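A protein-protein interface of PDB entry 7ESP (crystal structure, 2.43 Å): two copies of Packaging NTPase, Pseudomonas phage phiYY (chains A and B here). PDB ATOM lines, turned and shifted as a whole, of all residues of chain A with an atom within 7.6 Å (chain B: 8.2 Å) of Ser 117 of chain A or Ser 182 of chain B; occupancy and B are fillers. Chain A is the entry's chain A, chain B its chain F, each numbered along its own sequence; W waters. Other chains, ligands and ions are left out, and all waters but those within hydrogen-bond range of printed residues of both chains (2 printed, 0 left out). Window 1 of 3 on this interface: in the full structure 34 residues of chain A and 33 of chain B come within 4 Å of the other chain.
Of the printed residues of chain B, Ser 117 of chain A touches Gly 166, Ser 182 and Asn 208. Of chain A, only Leu 116, Ser 117 and Arg 119 come within 4 Å of Ser 182 of chain B. Printed residues of chain A within 4 Å of Gly 166 of chain B: Ser 117 (3.5 Å) and Thr 231 (3.8 Å). Of the printed residues of chain A, Trp 165 of chain B touches Leu 115 (3.3 Å). Val 236 of chain A touches none of the printed residues of chain B.
O of Ser 182 of chain B sits at hydrogen-bond distance from NE1 of Trp 165 of chain B (3.4 Å). The side-chain carboxylate (OD1) of Asp 183 of chain B is in hydrogen-bond range of the backbone NH (N) of Glu 186 of chain B (2.9 Å). The backbone carbonyl oxygen of Val 118 of chain A is in hydrogen-bond range of the side-chain amide nitrogen of Asn 235 of chain A.
The backbone NH (N) of Ser 117 of chain A is in hydrogen-bond range of the backbone carbonyl oxygen (O) of Ser 182 of chain B (2.6 Å). The side-chain hydroxyl of Thr 231 of chain A lies within hydrogen-bond range of the guanidinium group of Arg 207 of chain B (2.7 Å). O of Glu 167 of chain B sits at hydrogen-bond distance from ND2 of Asn 235 of chain A (2.8 Å). The backbone carbonyl oxygen of Leu 115 of chain A is in hydrogen-bond range of the side-chain amide nitrogen of Asn 208 of chain B (3.1 Å). The backbone carbonyl oxygen (O) of Pro 114 of chain A is in hydrogen-bond range of the backbone NH (N) of Leu 184 of chain B (3.0 Å).
Water W1 lies within hydrogen-bond range of N of Gly 166 of chain B, O of Val 118 of chain A, O of Val 181 of chain B and OG of Ser 117 of chain A. Water W2 lies within hydrogen-bond range of the guanidinium group of Arg 239 of chain A (2.7 Å), the backbone NH of Arg 119 of chain A (2.8 Å) and the side-chain hydroxyl of Ser 182 of chain B (3.0 Å).
No position is printed for both chains. Of the 24 pairs that touch across the chains among the printed residues, none has its exchanged pair printed and touching as well.
Among the printed residues, pairs that only touch across the chains: Tyr 113 of chain A with Asp 183 of chain B (3.4 Å), Pro 114 of chain A with Asp 183 of chain B (3.2 Å), Pro 114 of chain A with Asn 185 of chain B (3.2 Å), Leu 115 of chain A with Trp 165 of chain B (3.3 Å), Leu 116 of chain A with Ser 182 of chain B (3.5 Å), Leu 116 of chain A with Asn 208 of chain B (3.8 Å), Ser 117 of chain A with Gly 166 of chain B (3.5 Å), Ser 117 of chain A with Asn 208 of chain B (3.4 Å), Arg 119 of chain A with Ala 180 of chain B (3.8 Å), Arg 119 of chain A with Val 181 of chain B (3.3 Å), Arg 119 of chain A with Ser 182 of chain B (3.9 Å), Pro 120 of chain A with Arg 164 of chain B (3.8 Å), Pro 120 of chain A with Glu 167 of chain B (3.7 Å), Pro 120 of chain A with Ala 180 of chain B (3.3 Å), Ser 228 of chain A with Asn 208 of chain B (3.8 Å), Thr 231 of chain A with Gly 166 of chain B (3.8 Å), Thr 231 of chain A with Glu 167 of chain B (3.7 Å), Thr 231 of chain A with Pro 168 of chain B (3.8 Å) and Asn 235 of chain A with Pro 168 of chain B (3.4 Å).
Of the 18 printed residues of chain B, 13 touch a printed residue of chain A. Hydrophobic or aromatic side chains of chain B that line the printed part of chain A: Trp 165, Ala 180 and Leu 184. Along chain B the printed residues that touch a printed residue of chain A span positions 164 to 208. Printed residues of chain A that touch a printed residue of chain B: Tyr 113, Pro 114, Leu 115, Leu 116, Ser 117, Arg 119, Pro 120, Ser 228, Thr 231 and Asn 235. Hydrophobic or aromatic side chains of chain A within 4 Å of the printed part of chain B: Tyr 113, Pro 114, Leu 115, Leu 116 and Pro 120. Among the printed residues, no Asp or Glu carboxylate lies within 4 Å of a Lys or Arg side-chain nitrogen of the other chain.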
ATOM      1  N   ILE A  57      -9.667  -6.606 -22.453  1.00  0.00           N
ATOM      2  CA  ILE A  57      -8.476  -7.267 -22.982  1.00  0.00           C
ATOM      3  C   ILE A  57      -7.900  -8.180 -21.916  1.00  0.00           C
ATOM      4  O   ILE A  57      -7.685  -7.756 -20.772  1.00  0.00           O
ATOM      5  CB  ILE A  57      -7.423  -6.259 -23.467  1.00  0.00           C
ATOM      6  CG1 ILE A  57      -7.995  -5.428 -24.634  1.00  0.00           C
ATOM      7  CG2 ILE A  57      -6.165  -6.997 -23.905  1.00  0.00           C
ATOM      8  CD1 ILE A  57      -7.124  -4.228 -25.001  1.00  0.00           C
ATOM      9  N   MET A  58      -7.665  -9.437 -22.284  1.00  0.00           N
ATOM     10  CA  MET A  58      -7.156 -10.408 -21.333  1.00  0.00           C
ATOM     11  C   MET A  58      -5.638 -10.322 -21.296  1.00  0.00           C
ATOM     12  O   MET A  58      -4.991 -10.182 -22.337  1.00  0.00           O
ATOM     13  CB  MET A  58      -7.603 -11.819 -21.727  1.00  0.00           C
ATOM     14  CG  MET A  58      -8.943 -12.221 -21.109  1.00  0.00           C
ATOM     15  SD  MET A  58      -9.546 -13.874 -21.580  1.00  0.00           S
ATOM     16  CE  MET A  58      -9.381 -13.846 -23.365  1.00  0.00           C
ATOM     17  N   ILE A  59      -5.073 -10.417 -20.098  1.00  0.00           N
ATOM     18  CA  ILE A  59      -3.640 -10.295 -19.867  1.00  0.00           C
ATOM     19  C   ILE A  59      -3.156 -11.530 -19.117  1.00  0.00           C
ATOM     20  O   ILE A  59      -3.218 -11.586 -17.888  1.00  0.00           O
ATOM     21  CB  ILE A  59      -3.312  -9.025 -19.060  1.00  0.00           C
ATOM     22  CG1 ILE A  59      -4.022  -7.807 -19.631  1.00  0.00           C
ATOM     23  CG2 ILE A  59      -1.801  -8.837 -18.978  1.00  0.00           C
ATOM     24  CD1 ILE A  59      -3.977  -6.587 -18.713  1.00  0.00           C
ATOM     25  N   PRO A  60      -2.610 -12.526 -19.819  1.00  0.00           N
ATOM     26  CA  PRO A  60      -2.067 -13.715 -19.135  1.00  0.00           C
ATOM     27  C   PRO A  60      -0.708 -13.444 -18.487  1.00  0.00           C
ATOM     28  O   PRO A  60       0.220 -12.958 -19.130  1.00  0.00           O
ATOM     29  CB  PRO A  60      -1.938 -14.738 -20.267  1.00  0.00           C
ATOM     30  CG  PRO A  60      -1.673 -13.893 -21.474  1.00  0.00           C
ATOM     31  CD  PRO A  60      -2.478 -12.626 -21.280  1.00  0.00           C
ATOM     32  N   TYR A 113      -8.919 -20.395 -23.838  1.00  0.00           N
ATOM     33  CA  TYR A 113      -7.940 -19.581 -24.557  1.00  0.00           C
ATOM     34  C   TYR A 113      -6.562 -20.215 -24.379  1.00  0.00           C
ATOM     35  O   TYR A 113      -5.748 -19.769 -23.555  1.00  0.00           O
ATOM     36  CB  TYR A 113      -7.984 -18.139 -24.061  1.00  0.00           C
ATOM     37  CG  TYR A 113      -9.385 -17.600 -24.143  1.00  0.00           C
ATOM     38  CD1 TYR A 113      -9.926 -17.217 -25.363  1.00  0.00           C
ATOM     39  CD2 TYR A 113     -10.177 -17.501 -23.011  1.00  0.00           C
ATOM     40  CE1 TYR A 113     -11.217 -16.735 -25.456  1.00  0.00           C
ATOM     41  CE2 TYR A 113     -11.473 -17.005 -23.083  1.00  0.00           C
ATOM     42  CZ  TYR A 113     -11.989 -16.642 -24.313  1.00  0.00           C
ATOM     43  OH  TYR A 113     -13.287 -16.182 -24.392  1.00  0.00           O
ATOM     44  N   PRO A 114      -6.265 -21.257 -25.139  1.00  0.00           N
ATOM     45  CA  PRO A 114      -5.042 -22.024 -24.880  1.00  0.00           C
ATOM     46  C   PRO A 114      -3.810 -21.219 -25.264  1.00  0.00           C
ATOM     47  O   PRO A 114      -3.777 -20.583 -26.323  1.00  0.00           O
ATOM     48  CB  PRO A 114      -5.208 -23.271 -25.759  1.00  0.00           C
ATOM     49  CG  PRO A 114      -6.153 -22.847 -26.845  1.00  0.00           C
ATOM     50  CD  PRO A 114      -7.078 -21.822 -26.227  1.00  0.00           C
ATOM     51  N   LEU A 115      -2.804 -21.254 -24.387  1.00  0.00           N
ATOM     52  CA  LEU A 115      -1.521 -20.575 -24.581  1.00  0.00           C
ATOM     53  C   LEU A 115      -1.726 -19.097 -24.881  1.00  0.00           C
ATOM     54  O   LEU A 115      -1.063 -18.509 -25.738  1.00  0.00           O
ATOM     55  CB  LEU A 115      -0.686 -21.265 -25.666  1.00  0.00           C
ATOM     56  CG  LEU A 115      -0.381 -22.741 -25.301  1.00  0.00           C
ATOM     57  CD1 LEU A 115       0.325 -23.528 -26.424  1.00  0.00           C
ATOM     58  CD2 LEU A 115       0.409 -22.843 -24.007  1.00  0.00           C
ATOM     59  N   LEU A 116      -2.639 -18.489 -24.132  1.00  0.00           N
ATOM     60  CA  LEU A 116      -3.053 -17.120 -24.390  1.00  0.00           C
ATOM     61  C   LEU A 116      -1.875 -16.159 -24.274  1.00  0.00           C
ATOM     62  O   LEU A 116      -1.014 -16.297 -23.393  1.00  0.00           O
ATOM     63  CB  LEU A 116      -4.163 -16.735 -23.416  1.00  0.00           C
ATOM     64  CG  LEU A 116      -4.644 -15.280 -23.341  1.00  0.00           C
ATOM     65  CD1 LEU A 116      -5.392 -14.861 -24.579  1.00  0.00           C
ATOM     66  CD2 LEU A 116      -5.515 -15.080 -22.130  1.00  0.00           C
ATOM     67  N   SER A 117      -1.834 -15.205 -25.201  1.00  0.00           N
ATOM     68  CA  SER A 117      -0.901 -14.087 -25.168  1.00  0.00           C
ATOM     69  C   SER A 117      -1.750 -12.826 -25.361  1.00  0.00           C
ATOM     70  O   SER A 117      -2.957 -12.806 -25.075  1.00  0.00           O
ATOM     71  CB  SER A 117       0.194 -14.277 -26.224  1.00  0.00           C
ATOM     72  OG  SER A 117       1.062 -13.144 -26.287  1.00  0.00           O
ATOM     73  N   VAL A 118      -1.128 -11.725 -25.814  1.00  0.00           N
ATOM     74  CA  VAL A 118      -1.867 -10.519 -26.198  1.00  0.00           C
ATOM     75  C   VAL A 118      -1.463 -10.172 -27.626  1.00  0.00           C
ATOM     76  O   VAL A 118      -0.304 -10.364 -28.012  1.00  0.00           O
ATOM     77  CB  VAL A 118      -1.626  -9.345 -25.224  1.00  0.00           C
ATOM     78  CG1 VAL A 118      -2.396  -8.100 -25.628  1.00  0.00           C
ATOM     79  CG2 VAL A 118      -2.028  -9.733 -23.807  1.00  0.00           C
ATOM     80  N   ARG A 119      -2.420  -9.728 -28.436  1.00  0.00           N
ATOM     81  CA  ARG A 119      -1.992  -9.708 -29.836  1.00  0.00           C
ATOM     82  C   ARG A 119      -1.146  -8.468 -30.163  1.00  0.00           C
ATOM     83  O   ARG A 119      -1.448  -7.364 -29.697  1.00  0.00           O
ATOM     84  CB  ARG A 119      -3.204  -9.794 -30.765  1.00  0.00           C
ATOM     85  CG  ARG A 119      -3.994  -8.534 -30.941  1.00  0.00           C
ATOM     86  CD  ARG A 119      -5.404  -8.862 -31.435  1.00  0.00           C
ATOM     87  NE  ARG A 119      -6.119  -7.631 -31.747  1.00  0.00           N
ATOM     88  CZ  ARG A 119      -7.439  -7.505 -31.732  1.00  0.00           C
ATOM     89  NH1 ARG A 119      -8.190  -8.551 -31.397  1.00  0.00           N
ATOM     90  NH2 ARG A 119      -7.995  -6.326 -32.025  1.00  0.00           N
ATOM     91  N   PRO A 120      -0.066  -8.621 -30.975  1.00  0.00           N
ATOM     92  CA  PRO A 120       0.763  -7.455 -31.322  1.00  0.00           C
ATOM     93  C   PRO A 120       0.072  -6.518 -32.297  1.00  0.00           C
ATOM     94  O   PRO A 120      -0.020  -6.811 -33.493  1.00  0.00           O
ATOM     95  CB  PRO A 120       2.016  -8.078 -31.951  1.00  0.00           C
ATOM     96  CG  PRO A 120       1.564  -9.381 -32.470  1.00  0.00           C
ATOM     97  CD  PRO A 120       0.501  -9.872 -31.511  1.00  0.00           C
ATOM     98  N   SER A 228       7.272 -14.800 -21.234  1.00  0.00           N
ATOM     99  CA  SER A 228       5.978 -14.681 -21.889  1.00  0.00           C
ATOM    100  C   SER A 228       5.054 -13.736 -21.126  1.00  0.00           C
ATOM    101  O   SER A 228       4.226 -13.062 -21.743  1.00  0.00           O
ATOM    102  CB  SER A 228       5.359 -16.063 -22.067  1.00  0.00           C
ATOM    103  OG  SER A 228       5.007 -16.620 -20.814  1.00  0.00           O
ATOM    104  N   THR A 231       6.176 -10.315 -22.584  1.00  0.00           N
ATOM    105  CA  THR A 231       5.557 -10.083 -23.883  1.00  0.00           C
ATOM    106  C   THR A 231       4.072  -9.763 -23.743  1.00  0.00           C
ATOM    107  O   THR A 231       3.578  -8.832 -24.387  1.00  0.00           O
ATOM    108  CB  THR A 231       5.761 -11.282 -24.800  1.00  0.00           C
ATOM    109  OG1 THR A 231       7.167 -11.518 -24.960  1.00  0.00           O
ATOM    110  CG2 THR A 231       5.141 -10.978 -26.174  1.00  0.00           C
ATOM    111  N   ALA A 232       3.350 -10.506 -22.892  1.00  0.00           N
ATOM    112  CA  ALA A 232       1.926 -10.244 -22.687  1.00  0.00           C
ATOM    113  C   ALA A 232       1.692  -8.804 -22.284  1.00  0.00           C
ATOM    114  O   ALA A 232       0.917  -8.079 -22.930  1.00  0.00           O
ATOM    115  CB  ALA A 232       1.331 -11.178 -21.614  1.00  0.00           C
ATOM    116  N   ILE A 233       2.318  -8.388 -21.172  1.00  0.00           N
ATOM    117  CA  ILE A 233       2.137  -7.030 -20.650  1.00  0.00           C
ATOM    118  C   ILE A 233       2.626  -5.996 -21.663  1.00  0.00           C
ATOM    119  O   ILE A 233       2.014  -4.925 -21.825  1.00  0.00           O
ATOM    120  CB  ILE A 233       2.852  -6.889 -19.297  1.00  0.00           C
ATOM    121  CG1 ILE A 233       2.235  -7.867 -18.285  1.00  0.00           C
ATOM    122  CG2 ILE A 233       2.743  -5.456 -18.800  1.00  0.00           C
ATOM    123  CD1 ILE A 233       3.025  -8.046 -17.015  1.00  0.00           C
ATOM    124  N   ASN A 235       2.517  -6.279 -25.026  1.00  0.00           N
ATOM    125  CA  ASN A 235       1.550  -6.128 -26.103  1.00  0.00           C
ATOM    126  C   ASN A 235       0.239  -5.498 -25.640  1.00  0.00           C
ATOM    127  O   ASN A 235      -0.495  -4.958 -26.475  1.00  0.00           O
ATOM    128  CB  ASN A 235       1.319  -7.485 -26.781  1.00  0.00           C
ATOM    129  CG  ASN A 235       2.489  -7.874 -27.677  1.00  0.00           C
ATOM    130  OD1 ASN A 235       3.433  -7.112 -27.795  1.00  0.00           O
ATOM    131  ND2 ASN A 235       2.438  -9.052 -28.305  1.00  0.00           N
ATOM    132  N   VAL A 236      -0.064  -5.497 -24.338  1.00  0.00           N
ATOM    133  CA  VAL A 236      -1.197  -4.691 -23.887  1.00  0.00           C
ATOM    134  C   VAL A 236      -0.866  -3.209 -24.002  1.00  0.00           C
ATOM    135  O   VAL A 236      -1.672  -2.415 -24.506  1.00  0.00           O
ATOM    136  CB  VAL A 236      -1.617  -5.041 -22.448  1.00  0.00           C
ATOM    137  CG1 VAL A 236      -2.989  -4.427 -22.152  1.00  0.00           C
ATOM    138  CG2 VAL A 236      -1.660  -6.512 -22.249  1.00  0.00           C
ATOM    139  N   ARG A 239      -1.215  -2.433 -27.586  1.00  0.00           N
ATOM    140  CA  ARG A 239      -2.584  -2.201 -28.060  1.00  0.00           C
ATOM    141  C   ARG A 239      -3.130  -0.886 -27.546  1.00  0.00           C
ATOM    142  O   ARG A 239      -3.924  -0.239 -28.231  1.00  0.00           O
ATOM    143  CB  ARG A 239      -3.512  -3.324 -27.636  1.00  0.00           C
ATOM    144  CG  ARG A 239      -3.178  -4.630 -28.329  1.00  0.00           C
ATOM    145  CD  ARG A 239      -4.153  -5.705 -27.942  1.00  0.00           C
ATOM    146  NE  ARG A 239      -5.508  -5.352 -28.342  1.00  0.00           N
ATOM    147  CZ  ARG A 239      -6.563  -6.140 -28.171  1.00  0.00           C
ATOM    148  NH1 ARG A 239      -7.758  -5.710 -28.538  1.00  0.00           N
ATOM    149  NH2 ARG A 239      -6.422  -7.347 -27.622  1.00  0.00           N
ATOM    150  N   HIS B  98     -12.034 -17.395 -36.367  1.00  0.00           N
ATOM    151  CA  HIS B  98     -11.386 -17.815 -35.129  1.00  0.00           C
ATOM    152  C   HIS B  98     -12.131 -18.978 -34.469  1.00  0.00           C
ATOM    153  O   HIS B  98     -11.497 -19.841 -33.852  1.00  0.00           O
ATOM    154  CB  HIS B  98     -11.246 -16.613 -34.175  1.00  0.00           C
ATOM    155  CG  HIS B  98     -10.247 -15.579 -34.632  1.00  0.00           C
ATOM    156  ND1 HIS B  98     -10.074 -14.370 -33.989  1.00  0.00           N
ATOM    157  CD2 HIS B  98      -9.382 -15.568 -35.678  1.00  0.00           C
ATOM    158  CE1 HIS B  98      -9.143 -13.666 -34.612  1.00  0.00           C
ATOM    159  NE2 HIS B  98      -8.712 -14.366 -35.645  1.00  0.00           N
ATOM    160  N   ILE B 163       0.833 -14.727 -39.696  1.00  0.00           N
ATOM    161  CA  ILE B 163       0.011 -14.704 -38.495  1.00  0.00           C
ATOM    162  C   ILE B 163       0.935 -14.486 -37.301  1.00  0.00           C
ATOM    163  O   ILE B 163       1.842 -15.290 -37.038  1.00  0.00           O
ATOM    164  CB  ILE B 163      -0.787 -16.015 -38.352  1.00  0.00           C
ATOM    165  CG1 ILE B 163      -1.720 -16.217 -39.548  1.00  0.00           C
ATOM    166  CG2 ILE B 163      -1.623 -16.011 -37.091  1.00  0.00           C
ATOM    167  CD1 ILE B 163      -1.873 -17.643 -39.943  1.00  0.00           C
ATOM    168  N   ARG B 164       0.700 -13.419 -36.565  1.00  0.00           N
ATOM    169  CA  ARG B 164       1.618 -13.000 -35.517  1.00  0.00           C
ATOM    170  C   ARG B 164       1.029 -13.358 -34.160  1.00  0.00           C
ATOM    171  O   ARG B 164      -0.033 -12.855 -33.779  1.00  0.00           O
ATOM    172  CB  ARG B 164       1.922 -11.506 -35.621  1.00  0.00           C
ATOM    173  CG  ARG B 164       2.748 -11.184 -36.874  1.00  0.00           C
ATOM    174  CD  ARG B 164       4.257 -11.302 -36.621  1.00  0.00           C
ATOM    175  NE  ARG B 164       4.676 -10.322 -35.611  1.00  0.00           N
ATOM    176  CZ  ARG B 164       5.825 -10.373 -34.938  1.00  0.00           C
ATOM    177  NH1 ARG B 164       6.697 -11.351 -35.168  1.00  0.00           N
ATOM    178  NH2 ARG B 164       6.101  -9.444 -34.032  1.00  0.00           N
ATOM    179  N   TRP B 165       1.740 -14.201 -33.429  1.00  0.00           N
ATOM    180  CA  TRP B 165       1.250 -14.735 -32.179  1.00  0.00           C
ATOM    181  C   TRP B 165       2.393 -14.788 -31.174  1.00  0.00           C
ATOM    182  O   TRP B 165       3.434 -15.379 -31.462  1.00  0.00           O
ATOM    183  CB  TRP B 165       0.659 -16.132 -32.405  1.00  0.00           C
ATOM    184  CG  TRP B 165       0.191 -16.742 -31.162  1.00  0.00           C
ATOM    185  CD1 TRP B 165      -0.545 -16.139 -30.159  1.00  0.00           C
ATOM    186  CD2 TRP B 165       0.402 -18.090 -30.762  1.00  0.00           C
ATOM    187  NE1 TRP B 165      -0.786 -17.044 -29.158  1.00  0.00           N
ATOM    188  CE2 TRP B 165      -0.224 -18.252 -29.505  1.00  0.00           C
ATOM    189  CE3 TRP B 165       1.076 -19.175 -31.337  1.00  0.00           C
ATOM    190  CZ2 TRP B 165      -0.184 -19.461 -28.805  1.00  0.00           C
ATOM    191  CZ3 TRP B 165       1.114 -20.378 -30.649  1.00  0.00           C
ATOM    192  CH2 TRP B 165       0.490 -20.510 -29.384  1.00  0.00           C
ATOM    193  N   GLY B 166       2.193 -14.187 -29.999  1.00  0.00           N
ATOM    194  CA  GLY B 166       3.125 -14.375 -28.900  1.00  0.00           C
ATOM    195  C   GLY B 166       4.475 -13.699 -29.040  1.00  0.00           C
ATOM    196  O   GLY B 166       5.423 -14.083 -28.355  1.00  0.00           O
ATOM    197  N   GLU B 167       4.585 -12.694 -29.894  1.00  0.00           N
ATOM    198  CA  GLU B 167       5.807 -11.971 -30.137  1.00  0.00           C
ATOM    199  C   GLU B 167       5.568 -10.497 -29.854  1.00  0.00           C
ATOM    200  O   GLU B 167       4.429 -10.023 -29.993  1.00  0.00           O
ATOM    201  CB  GLU B 167       6.248 -12.166 -31.590  1.00  0.00           C
ATOM    202  CG  GLU B 167       6.663 -13.586 -31.901  1.00  0.00           C
ATOM    203  CD  GLU B 167       8.015 -13.936 -31.288  1.00  0.00           C
ATOM    204  OE1 GLU B 167       8.632 -13.050 -30.653  1.00  0.00           O
ATOM    205  OE2 GLU B 167       8.450 -15.100 -31.424  1.00  0.00           O
ATOM    206  N   PRO B 168       6.598  -9.755 -29.420  1.00  0.00           N
ATOM    207  CA  PRO B 168       6.386  -8.332 -29.095  1.00  0.00           C
ATOM    208  C   PRO B 168       6.131  -7.539 -30.359  1.00  0.00           C
ATOM    209  O   PRO B 168       6.734  -7.797 -31.398  1.00  0.00           O
ATOM    210  CB  PRO B 168       7.700  -7.907 -28.407  1.00  0.00           C
ATOM    211  CG  PRO B 168       8.723  -8.950 -28.828  1.00  0.00           C
ATOM    212  CD  PRO B 168       7.959 -10.221 -29.077  1.00  0.00           C
ATOM    213  N   HIS B 179      -1.561 -10.632 -39.682  1.00  0.00           N
ATOM    214  CA  HIS B 179      -2.774 -10.768 -38.887  1.00  0.00           C
ATOM    215  C   HIS B 179      -2.368 -11.154 -37.479  1.00  0.00           C
ATOM    216  O   HIS B 179      -1.729 -12.192 -37.281  1.00  0.00           O
ATOM    217  CB  HIS B 179      -3.739 -11.797 -39.487  1.00  0.00           C
ATOM    218  CG  HIS B 179      -5.032 -11.862 -38.755  1.00  0.00           C
ATOM    219  ND1 HIS B 179      -5.880 -10.780 -38.658  1.00  0.00           N
ATOM    220  CD2 HIS B 179      -5.585 -12.844 -38.004  1.00  0.00           C
ATOM    221  CE1 HIS B 179      -6.917 -11.105 -37.910  1.00  0.00           C
ATOM    222  NE2 HIS B 179      -6.754 -12.347 -37.489  1.00  0.00           N
ATOM    223  N   ALA B 180      -2.700 -10.307 -36.510  1.00  0.00           N
ATOM    224  CA  ALA B 180      -2.338 -10.553 -35.127  1.00  0.00           C
ATOM    225  C   ALA B 180      -3.433 -11.347 -34.417  1.00  0.00           C
ATOM    226  O   ALA B 180      -4.621 -11.024 -34.539  1.00  0.00           O
ATOM    227  CB  ALA B 180      -2.099  -9.229 -34.398  1.00  0.00           C
ATOM    228  N   VAL B 181      -3.019 -12.373 -33.651  1.00  0.00           N
ATOM    229  CA  VAL B 181      -3.922 -13.219 -32.866  1.00  0.00           C
ATOM    230  C   VAL B 181      -3.403 -13.324 -31.429  1.00  0.00           C
ATOM    231  O   VAL B 181      -2.282 -12.920 -31.118  1.00  0.00           O
ATOM    232  CB  VAL B 181      -4.095 -14.631 -33.475  1.00  0.00           C
ATOM    233  CG1 VAL B 181      -4.613 -14.552 -34.900  1.00  0.00           C
ATOM    234  CG2 VAL B 181      -2.783 -15.385 -33.448  1.00  0.00           C
ATOM    235  N   SER B 182      -4.239 -13.907 -30.555  1.00  0.00           N
ATOM    236  CA  SER B 182      -4.034 -13.969 -29.110  1.00  0.00           C
ATOM    237  C   SER B 182      -3.782 -15.359 -28.540  1.00  0.00           C
ATOM    238  O   SER B 182      -3.236 -15.439 -27.428  1.00  0.00           O
ATOM    239  CB  SER B 182      -5.264 -13.430 -28.359  1.00  0.00           C
ATOM    240  OG  SER B 182      -5.552 -12.114 -28.749  1.00  0.00           O
ATOM    241  N   ASP B 183      -4.257 -16.440 -29.185  1.00  0.00           N
ATOM    242  CA  ASP B 183      -4.132 -17.779 -28.600  1.00  0.00           C
ATOM    243  C   ASP B 183      -3.979 -18.808 -29.705  1.00  0.00           C
ATOM    244  O   ASP B 183      -4.071 -18.489 -30.892  1.00  0.00           O
ATOM    245  CB  ASP B 183      -5.306 -18.139 -27.668  1.00  0.00           C
ATOM    246  CG  ASP B 183      -6.667 -18.177 -28.376  1.00  0.00           C
ATOM    247  OD1 ASP B 183      -6.816 -18.706 -29.520  1.00  0.00           O
ATOM    248  OD2 ASP B 183      -7.620 -17.689 -27.747  1.00  0.00           O
ATOM    249  N   LEU B 184      -3.689 -20.051 -29.303  1.00  0.00           N
ATOM    250  CA  LEU B 184      -3.384 -21.100 -30.280  1.00  0.00           C
ATOM    251  C   LEU B 184      -4.594 -21.448 -31.149  1.00  0.00           C
ATOM    252  O   LEU B 184      -4.430 -21.775 -32.330  1.00  0.00           O
ATOM    253  CB  LEU B 184      -2.869 -22.341 -29.556  1.00  0.00           C
ATOM    254  CG  LEU B 184      -2.483 -23.569 -30.400  1.00  0.00           C
ATOM    255  CD1 LEU B 184      -1.465 -23.182 -31.494  1.00  0.00           C
ATOM    256  CD2 LEU B 184      -1.937 -24.690 -29.520  1.00  0.00           C
ATOM    257  N   ASN B 185      -5.809 -21.382 -30.585  1.00  0.00           N
ATOM    258  CA  ASN B 185      -7.032 -21.581 -31.364  1.00  0.00           C
ATOM    259  C   ASN B 185      -7.082 -20.637 -32.557  1.00  0.00           C
ATOM    260  O   ASN B 185      -7.295 -21.069 -33.701  1.00  0.00           O
ATOM    261  CB  ASN B 185      -8.270 -21.352 -30.484  1.00  0.00           C
ATOM    262  CG  ASN B 185      -8.538 -22.502 -29.515  1.00  0.00           C
ATOM    263  OD1 ASN B 185      -8.033 -23.630 -29.672  1.00  0.00           O
ATOM    264  ND2 ASN B 185      -9.350 -22.217 -28.502  1.00  0.00           N
ATOM    265  N   GLU B 186      -6.897 -19.331 -32.301  1.00  0.00           N
ATOM    266  CA  GLU B 186      -6.946 -18.360 -33.386  1.00  0.00           C
ATOM    267  C   GLU B 186      -5.811 -18.586 -34.371  1.00  0.00           C
ATOM    268  O   GLU B 186      -6.041 -18.594 -35.585  1.00  0.00           O
ATOM    269  CB  GLU B 186      -6.903 -16.932 -32.840  1.00  0.00           C
ATOM    270  CG  GLU B 186      -7.969 -16.626 -31.816  1.00  0.00           C
ATOM    271  CD  GLU B 186      -7.769 -15.260 -31.180  1.00  0.00           C
ATOM    272  OE1 GLU B 186      -8.726 -14.706 -30.578  1.00  0.00           O
ATOM    273  OE2 GLU B 186      -6.644 -14.728 -31.300  1.00  0.00           O
ATOM    274  N   ALA B 187      -4.586 -18.807 -33.879  1.00  0.00           N
ATOM    275  CA  ALA B 187      -3.467 -19.013 -34.797  1.00  0.00           C
ATOM    276  C   ALA B 187      -3.736 -20.197 -35.716  1.00  0.00           C
ATOM    277  O   ALA B 187      -3.528 -20.102 -36.933  1.00  0.00           O
ATOM    278  CB  ALA B 187      -2.163 -19.227 -34.030  1.00  0.00           C
ATOM    279  N   ARG B 207       6.348 -19.575 -30.286  1.00  0.00           N
ATOM    280  CA  ARG B 207       7.085 -19.264 -29.072  1.00  0.00           C
ATOM    281  C   ARG B 207       6.332 -19.696 -27.811  1.00  0.00           C
ATOM    282  O   ARG B 207       6.936 -20.263 -26.890  1.00  0.00           O
ATOM    283  CB  ARG B 207       7.386 -17.772 -29.033  1.00  0.00           C
ATOM    284  CG  ARG B 207       7.739 -17.260 -27.664  1.00  0.00           C
ATOM    285  CD  ARG B 207       8.485 -15.959 -27.800  1.00  0.00           C
ATOM    286  NE  ARG B 207       8.203 -15.096 -26.659  1.00  0.00           N
ATOM    287  CZ  ARG B 207       9.131 -14.385 -26.046  1.00  0.00           C
ATOM    288  NH1 ARG B 207      10.383 -14.472 -26.473  1.00  0.00           N
ATOM    289  NH2 ARG B 207       8.817 -13.623 -25.002  1.00  0.00           N
ATOM    290  N   ASN B 208       5.015 -19.431 -27.723  1.00  0.00           N
ATOM    291  CA  ASN B 208       4.331 -19.864 -26.502  1.00  0.00           C
ATOM    292  C   ASN B 208       4.139 -21.363 -26.386  1.00  0.00           C
ATOM    293  O   ASN B 208       3.912 -21.827 -25.268  1.00  0.00           O
ATOM    294  CB  ASN B 208       2.944 -19.273 -26.275  1.00  0.00           C
ATOM    295  CG  ASN B 208       2.974 -17.817 -25.919  1.00  0.00           C
ATOM    296  OD1 ASN B 208       3.988 -17.314 -25.428  1.00  0.00           O
ATOM    297  ND2 ASN B 208       1.791 -17.231 -25.844  1.00  0.00           N
HETATM  298  O   HOH W   1       0.090 -12.699 -29.339  1.00  0.00           O
HETATM  299  O   HOH W   2      -4.970  -9.631 -27.261  1.00  0.00           O
